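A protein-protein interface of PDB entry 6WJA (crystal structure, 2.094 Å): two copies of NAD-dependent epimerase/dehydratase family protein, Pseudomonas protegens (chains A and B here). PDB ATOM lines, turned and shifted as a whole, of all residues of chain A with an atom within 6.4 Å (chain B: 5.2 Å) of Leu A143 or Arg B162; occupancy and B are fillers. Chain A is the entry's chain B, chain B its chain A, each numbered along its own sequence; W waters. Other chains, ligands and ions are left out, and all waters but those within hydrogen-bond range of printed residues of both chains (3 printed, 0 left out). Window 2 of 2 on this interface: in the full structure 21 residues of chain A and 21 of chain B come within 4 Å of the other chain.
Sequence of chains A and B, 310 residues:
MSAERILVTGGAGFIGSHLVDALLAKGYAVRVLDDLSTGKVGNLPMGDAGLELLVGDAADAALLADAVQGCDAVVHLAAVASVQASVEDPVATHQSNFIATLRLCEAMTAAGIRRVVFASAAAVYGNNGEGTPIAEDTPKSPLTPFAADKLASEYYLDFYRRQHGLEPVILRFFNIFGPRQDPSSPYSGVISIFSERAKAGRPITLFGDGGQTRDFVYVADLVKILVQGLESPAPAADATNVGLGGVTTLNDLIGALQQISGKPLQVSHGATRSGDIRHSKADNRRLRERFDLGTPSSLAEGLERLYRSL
Water W2 lies within hydrogen-bond range of a ring nitrogen (NE2) of His B164 (2.5 Å) and the backbone carbonyl oxygen (O) of Val A87 (3.0 Å). Water W3 bridges the backbone carbonyl oxygen of Leu A143 (2.6 Å) and the guanidinium group of Arg B162 (2.9 Å). Water W1 lies within hydrogen-bond range of the backbone carbonyl oxygen (O) of Pro A142 (2.6 Å), the backbone carbonyl oxygen (O) of Tyr B155 (2.8 Å) and the guanidinium group (NH1) of Arg B162 (2.8 Å).
OD2 of Asp B158 lies within salt-bridge range of NE of Arg B162, at 2.8 Å.
Of the printed residues of chain B, Val A87 touches Phe B159 (3.9 Å) and Gln B163 (3.9 Å). Leu A143 touches just these residues of chain B: Phe B159 and Arg B162. Of the printed residues of chain B, Ala A148 touches Tyr B155 (3.995 Å). Printed residues of chain A within 4 Å of Tyr B155: Pro A142 and Ala A148. Of the printed residues of chain A, Gln B163 touches Val A87. The nearest residue of chain A that does not touch Arg B162 is Pro A142 (4.4 Å).
The backbone carbonyl oxygen (O) of Leu A143 sits at hydrogen-bond distance from the guanidinium group (NH1) of Arg B162 (3.1 Å).
Printed residues of chain A that touch a printed residue of chain B: Val A87, Pro A142, Leu A143, Pro A145 and Ala A148. Hydrophobic or aromatic side chains of chain A that line the printed part of chain B: Val A87, Pro A142, Leu A143, Pro A145 and Ala A148. Printed residues of chain B that touch a printed residue of chain A: Tyr B155, Phe B159, Arg B162 and Gln B163. Hydrophobic or aromatic side chains of chain B within 4 Å of the printed part of chain A: Tyr B155 and Phe B159.
No position is printed for both chains. Of the 7 pairs that touch across the chains among the printed residues, none has its exchanged pair printed and touching as well.
CZ of Phe B159 touches O of Val A87, 3.9 Å away. Gln B163 touches Val A87. CG of Pro A142 touches CD2 of Tyr B155 (3.5 Å). Leu A143 touches Phe B159 (O to CD1, 3.4 Å). Phe B159 touches Pro A145. Ala A148 touches Tyr B155.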
ATOM      1  N   VAL A  87      27.835  -1.229   7.970  1.00  0.00           N
ATOM      2  CA  VAL A  87      27.764  -1.810   9.306  1.00  0.00           C
ATOM      3  C   VAL A  87      28.543  -3.116   9.350  1.00  0.00           C
ATOM      4  O   VAL A  87      29.204  -3.433  10.345  1.00  0.00           O
ATOM      5  CB  VAL A  87      26.293  -2.000   9.720  1.00  0.00           C
ATOM      6  CG1 VAL A  87      26.200  -2.797  11.008  1.00  0.00           C
ATOM      7  CG2 VAL A  87      25.604  -0.629   9.885  1.00  0.00           C
ATOM      8  N   ALA A 123      20.937  10.656   6.464  1.00  0.00           N
ATOM      9  CA  ALA A 123      21.441   9.818   7.546  1.00  0.00           C
ATOM     10  C   ALA A 123      22.360  10.578   8.506  1.00  0.00           C
ATOM     11  O   ALA A 123      22.558  10.117   9.634  1.00  0.00           O
ATOM     12  CB  ALA A 123      22.173   8.593   6.972  1.00  0.00           C
ATOM     13  N   VAL A 124      22.888  11.742   8.125  1.00  0.00           N
ATOM     14  CA  VAL A 124      23.778  12.442   9.068  1.00  0.00           C
ATOM     15  C   VAL A 124      23.011  12.977  10.278  1.00  0.00           C
ATOM     16  O   VAL A 124      23.609  13.198  11.340  1.00  0.00           O
ATOM     17  CB  VAL A 124      24.568  13.588   8.394  1.00  0.00           C
ATOM     18  CG1 VAL A 124      25.332  13.088   7.147  1.00  0.00           C
ATOM     19  CG2 VAL A 124      23.669  14.738   8.033  1.00  0.00           C
ATOM     20  N   GLY A 126      20.792  11.215  11.878  1.00  0.00           N
ATOM     21  CA  GLY A 126      20.380  10.124  12.749  1.00  0.00           C
ATOM     22  C   GLY A 126      18.914  10.266  13.129  1.00  0.00           C
ATOM     23  O   GLY A 126      18.050  10.547  12.284  1.00  0.00           O
ATOM     24  N   ASN A 127      18.627  10.092  14.421  1.00  0.00           N
ATOM     25  CA  ASN A 127      17.278  10.235  14.956  1.00  0.00           C
ATOM     26  C   ASN A 127      16.931  11.658  15.383  1.00  0.00           C
ATOM     27  O   ASN A 127      15.811  11.883  15.859  1.00  0.00           O
ATOM     28  CB  ASN A 127      17.075   9.295  16.154  1.00  0.00           C
ATOM     29  CG  ASN A 127      16.605   7.925  15.738  1.00  0.00           C
ATOM     30  OD1 ASN A 127      17.406   7.072  15.349  1.00  0.00           O
ATOM     31  ND2 ASN A 127      15.294   7.701  15.814  1.00  0.00           N
ATOM     32  N   SER A 141      23.832  13.351  14.114  1.00  0.00           N
ATOM     33  CA  SER A 141      23.979  12.151  14.924  1.00  0.00           C
ATOM     34  C   SER A 141      24.158  10.926  14.038  1.00  0.00           C
ATOM     35  O   SER A 141      23.294  10.043  14.030  1.00  0.00           O
ATOM     36  CB  SER A 141      22.766  11.984  15.840  1.00  0.00           C
ATOM     37  OG  SER A 141      22.986  10.945  16.768  1.00  0.00           O
ATOM     38  N   PRO A 142      25.248  10.841  13.268  1.00  0.00           N
ATOM     39  CA  PRO A 142      25.428   9.683  12.386  1.00  0.00           C
ATOM     40  C   PRO A 142      25.588   8.403  13.195  1.00  0.00           C
ATOM     41  O   PRO A 142      26.422   8.322  14.100  1.00  0.00           O
ATOM     42  CB  PRO A 142      26.698  10.033  11.601  1.00  0.00           C
ATOM     43  CG  PRO A 142      27.427  10.996  12.467  1.00  0.00           C
ATOM     44  CD  PRO A 142      26.379  11.787  13.181  1.00  0.00           C
ATOM     45  N   LEU A 143      24.778   7.393  12.859  1.00  0.00           N
ATOM     46  CA  LEU A 143      24.701   6.158  13.635  1.00  0.00           C
ATOM     47  C   LEU A 143      25.462   4.996  13.012  1.00  0.00           C
ATOM     48  O   LEU A 143      25.605   3.959  13.663  1.00  0.00           O
ATOM     49  CB  LEU A 143      23.223   5.744  13.846  1.00  0.00           C
ATOM     50  CG  LEU A 143      22.351   6.732  14.627  1.00  0.00           C
ATOM     51  CD1 LEU A 143      20.884   6.289  14.613  1.00  0.00           C
ATOM     52  CD2 LEU A 143      22.857   6.891  16.066  1.00  0.00           C
ATOM     53  N   THR A 144      25.974   5.145  11.798  1.00  0.00           N
ATOM     54  CA  THR A 144      26.649   4.079  11.076  1.00  0.00           C
ATOM     55  C   THR A 144      27.918   4.631  10.456  1.00  0.00           C
ATOM     56  O   THR A 144      28.079   5.853  10.342  1.00  0.00           O
ATOM     57  CB  THR A 144      25.750   3.497   9.976  1.00  0.00           C
ATOM     58  OG1 THR A 144      25.415   4.540   9.056  1.00  0.00           O
ATOM     59  CG2 THR A 144      24.473   2.900  10.577  1.00  0.00           C
ATOM     60  N   PRO A 145      28.851   3.766  10.047  1.00  0.00           N
ATOM     61  CA  PRO A 145      30.042   4.275   9.340  1.00  0.00           C
ATOM     62  C   PRO A 145      29.703   5.039   8.069  1.00  0.00           C
ATOM     63  O   PRO A 145      30.341   6.061   7.793  1.00  0.00           O
ATOM     64  CB  PRO A 145      30.847   2.997   9.055  1.00  0.00           C
ATOM     65  CG  PRO A 145      30.445   2.069  10.154  1.00  0.00           C
ATOM     66  CD  PRO A 145      28.982   2.339  10.386  1.00  0.00           C
ATOM     67  N   ALA A 147      27.014   6.887   7.557  1.00  0.00           N
ATOM     68  CA  ALA A 147      26.520   8.217   7.889  1.00  0.00           C
ATOM     69  C   ALA A 147      27.647   9.106   8.397  1.00  0.00           C
ATOM     70  O   ALA A 147      27.717  10.288   8.047  1.00  0.00           O
ATOM     71  CB  ALA A 147      25.384   8.121   8.921  1.00  0.00           C
ATOM     72  N   ALA A 148      28.540   8.554   9.223  1.00  0.00           N
ATOM     73  CA  ALA A 148      29.675   9.325   9.710  1.00  0.00           C
ATOM     74  C   ALA A 148      30.635   9.675   8.574  1.00  0.00           C
ATOM     75  O   ALA A 148      31.284  10.729   8.611  1.00  0.00           O
ATOM     76  CB  ALA A 148      30.397   8.539  10.807  1.00  0.00           C
ATOM     77  N   GLY A 275      17.242  -0.814  12.732  1.00  0.00           N
ATOM     78  CA  GLY A 275      17.745   0.548  12.663  1.00  0.00           C
ATOM     79  C   GLY A 275      16.752   1.556  12.117  1.00  0.00           C
ATOM     80  O   GLY A 275      17.143   2.653  11.708  1.00  0.00           O
ATOM     81  N   ILE A 277      14.243   4.371  11.315  1.00  0.00           N
ATOM     82  CA  ILE A 277      13.677   5.650  11.733  1.00  0.00           C
ATOM     83  C   ILE A 277      12.216   5.690  11.305  1.00  0.00           C
ATOM     84  O   ILE A 277      11.896   5.440  10.137  1.00  0.00           O
ATOM     85  CB  ILE A 277      14.465   6.817  11.125  1.00  0.00           C
ATOM     86  CG1 ILE A 277      15.907   6.794  11.642  1.00  0.00           C
ATOM     87  CG2 ILE A 277      13.797   8.146  11.459  1.00  0.00           C
ATOM     88  CD1 ILE A 277      16.789   7.861  11.038  1.00  0.00           C
ATOM     89  N   TYR B 155      32.316   9.411  16.568  1.00  0.00           N
ATOM     90  CA  TYR B 155      31.133   8.775  15.995  1.00  0.00           C
ATOM     91  C   TYR B 155      31.358   7.283  15.781  1.00  0.00           C
ATOM     92  O   TYR B 155      30.460   6.471  16.040  1.00  0.00           O
ATOM     93  CB  TYR B 155      30.753   9.458  14.679  1.00  0.00           C
ATOM     94  CG  TYR B 155      30.214  10.870  14.862  1.00  0.00           C
ATOM     95  CD1 TYR B 155      29.417  11.194  15.950  1.00  0.00           C
ATOM     96  CD2 TYR B 155      30.511  11.871  13.951  1.00  0.00           C
ATOM     97  CE1 TYR B 155      28.924  12.477  16.120  1.00  0.00           C
ATOM     98  CE2 TYR B 155      30.024  13.160  14.115  1.00  0.00           C
ATOM     99  CZ  TYR B 155      29.235  13.455  15.199  1.00  0.00           C
ATOM    100  OH  TYR B 155      28.747  14.731  15.357  1.00  0.00           O
ATOM    101  N   ASP B 158      31.211   5.460  19.090  1.00  0.00           N
ATOM    102  CA  ASP B 158      29.827   5.268  19.525  1.00  0.00           C
ATOM    103  C   ASP B 158      29.148   4.149  18.742  1.00  0.00           C
ATOM    104  O   ASP B 158      28.323   3.407  19.296  1.00  0.00           O
ATOM    105  CB  ASP B 158      29.024   6.568  19.374  1.00  0.00           C
ATOM    106  CG  ASP B 158      27.600   6.425  19.901  1.00  0.00           C
ATOM    107  OD1 ASP B 158      27.447   6.299  21.131  1.00  0.00           O
ATOM    108  OD2 ASP B 158      26.647   6.391  19.094  1.00  0.00           O
ATOM    109  N   PHE B 159      29.451   4.034  17.446  1.00  0.00           N
ATOM    110  CA  PHE B 159      28.910   2.922  16.667  1.00  0.00           C
ATOM    111  C   PHE B 159      29.422   1.578  17.183  1.00  0.00           C
ATOM    112  O   PHE B 159      28.669   0.599  17.237  1.00  0.00           O
ATOM    113  CB  PHE B 159      29.251   3.085  15.185  1.00  0.00           C
ATOM    114  CG  PHE B 159      29.102   1.817  14.397  1.00  0.00           C
ATOM    115  CD1 PHE B 159      27.848   1.365  14.014  1.00  0.00           C
ATOM    116  CD2 PHE B 159      30.214   1.063  14.059  1.00  0.00           C
ATOM    117  CE1 PHE B 159      27.709   0.183  13.299  1.00  0.00           C
ATOM    118  CE2 PHE B 159      30.080  -0.122  13.354  1.00  0.00           C
ATOM    119  CZ  PHE B 159      28.832  -0.561  12.969  1.00  0.00           C
ATOM    120  N   TYR B 160      30.706   1.494  17.541  1.00  0.00           N
ATOM    121  CA  TYR B 160      31.210   0.232  18.081  1.00  0.00           C
ATOM    122  C   TYR B 160      30.633  -0.049  19.465  1.00  0.00           C
ATOM    123  O   TYR B 160      30.449  -1.217  19.833  1.00  0.00           O
ATOM    124  CB  TYR B 160      32.737   0.244  18.114  1.00  0.00           C
ATOM    125  CG  TYR B 160      33.353  -0.176  16.798  1.00  0.00           C
ATOM    126  CD1 TYR B 160      33.555   0.743  15.776  1.00  0.00           C
ATOM    127  CD2 TYR B 160      33.718  -1.496  16.574  1.00  0.00           C
ATOM    128  CE1 TYR B 160      34.127   0.364  14.574  1.00  0.00           C
ATOM    129  CE2 TYR B 160      34.285  -1.890  15.370  1.00  0.00           C
ATOM    130  CZ  TYR B 160      34.482  -0.955  14.375  1.00  0.00           C
ATOM    131  OH  TYR B 160      35.038  -1.341  13.179  1.00  0.00           O
ATOM    132  N   ARG B 161      30.318   0.999  20.233  1.00  0.00           N
ATOM    133  CA  ARG B 161      29.634   0.798  21.509  1.00  0.00           C
ATOM    134  C   ARG B 161      28.276   0.135  21.303  1.00  0.00           C
ATOM    135  O   ARG B 161      27.966  -0.884  21.929  1.00  0.00           O
ATOM    136  CB  ARG B 161      29.469   2.135  22.249  1.00  0.00           C
ATOM    137  CG  ARG B 161      28.555   2.016  23.480  1.00  0.00           C
ATOM    138  CD  ARG B 161      28.305   3.364  24.154  1.00  0.00           C
ATOM    139  NE  ARG B 161      27.474   4.253  23.343  1.00  0.00           N
ATOM    140  CZ  ARG B 161      26.143   4.210  23.304  1.00  0.00           C
ATOM    141  NH1 ARG B 161      25.485   3.315  24.027  1.00  0.00           N
ATOM    142  NH2 ARG B 161      25.470   5.064  22.543  1.00  0.00           N
ATOM    143  N   ARG B 162      27.455   0.698  20.416  1.00  0.00           N
ATOM    144  CA  ARG B 162      26.097   0.186  20.231  1.00  0.00           C
ATOM    145  C   ARG B 162      26.092  -1.134  19.467  1.00  0.00           C
ATOM    146  O   ARG B 162      25.266  -2.009  19.739  1.00  0.00           O
ATOM    147  CB  ARG B 162      25.242   1.223  19.499  1.00  0.00           C
ATOM    148  CG  ARG B 162      24.839   2.421  20.343  1.00  0.00           C
ATOM    149  CD  ARG B 162      24.025   3.436  19.534  1.00  0.00           C
ATOM    150  NE  ARG B 162      24.885   4.223  18.657  1.00  0.00           N
ATOM    151  CZ  ARG B 162      25.031   4.009  17.349  1.00  0.00           C
ATOM    152  NH1 ARG B 162      25.852   4.773  16.633  1.00  0.00           N
ATOM    153  NH2 ARG B 162      24.348   3.050  16.753  1.00  0.00           N
ATOM    154  N   GLN B 163      26.995  -1.298  18.500  1.00  0.00           N
ATOM    155  CA  GLN B 163      26.967  -2.485  17.651  1.00  0.00           C
ATOM    156  C   GLN B 163      27.830  -3.631  18.178  1.00  0.00           C
ATOM    157  O   GLN B 163      27.532  -4.797  17.892  1.00  0.00           O
ATOM    158  CB  GLN B 163      27.408  -2.123  16.226  1.00  0.00           C
ATOM    159  CG  GLN B 163      27.249  -3.247  15.206  1.00  0.00           C
ATOM    160  CD  GLN B 163      25.798  -3.505  14.824  1.00  0.00           C
ATOM    161  OE1 GLN B 163      24.987  -2.585  14.747  1.00  0.00           O
ATOM    162  NE2 GLN B 163      25.469  -4.762  14.583  1.00  0.00           N
ATOM    163  N   HIS B 164      28.874  -3.348  18.961  1.00  0.00           N
ATOM    164  CA  HIS B 164      29.807  -4.398  19.355  1.00  0.00           C
ATOM    165  C   HIS B 164      30.172  -4.385  20.838  1.00  0.00           C
ATOM    166  O   HIS B 164      31.095  -5.099  21.240  1.00  0.00           O
ATOM    167  CB  HIS B 164      31.071  -4.308  18.487  1.00  0.00           C
ATOM    168  CG  HIS B 164      30.809  -4.510  17.024  1.00  0.00           C
ATOM    169  ND1 HIS B 164      30.344  -5.701  16.506  1.00  0.00           N
ATOM    170  CD2 HIS B 164      30.943  -3.671  15.969  1.00  0.00           C
ATOM    171  CE1 HIS B 164      30.203  -5.588  15.197  1.00  0.00           C
ATOM    172  NE2 HIS B 164      30.556  -4.364  14.846  1.00  0.00           N
ATOM    173  N   GLY B 165      29.473  -3.618  21.669  1.00  0.00           N
ATOM    174  CA  GLY B 165      29.694  -3.685  23.104  1.00  0.00           C
ATOM    175  C   GLY B 165      30.917  -2.953  23.622  1.00  0.00           C
ATOM    176  O   GLY B 165      31.265  -3.123  24.795  1.00  0.00           O
HETATM  177  O   HOH W   1      27.761   6.445  15.387  1.00  0.00           O
HETATM  178  O   HOH W   2      31.269  -3.598  12.545  1.00  0.00           O
HETATM  179  O   HOH W   3      23.850   2.093  14.045  1.00  0.00           O
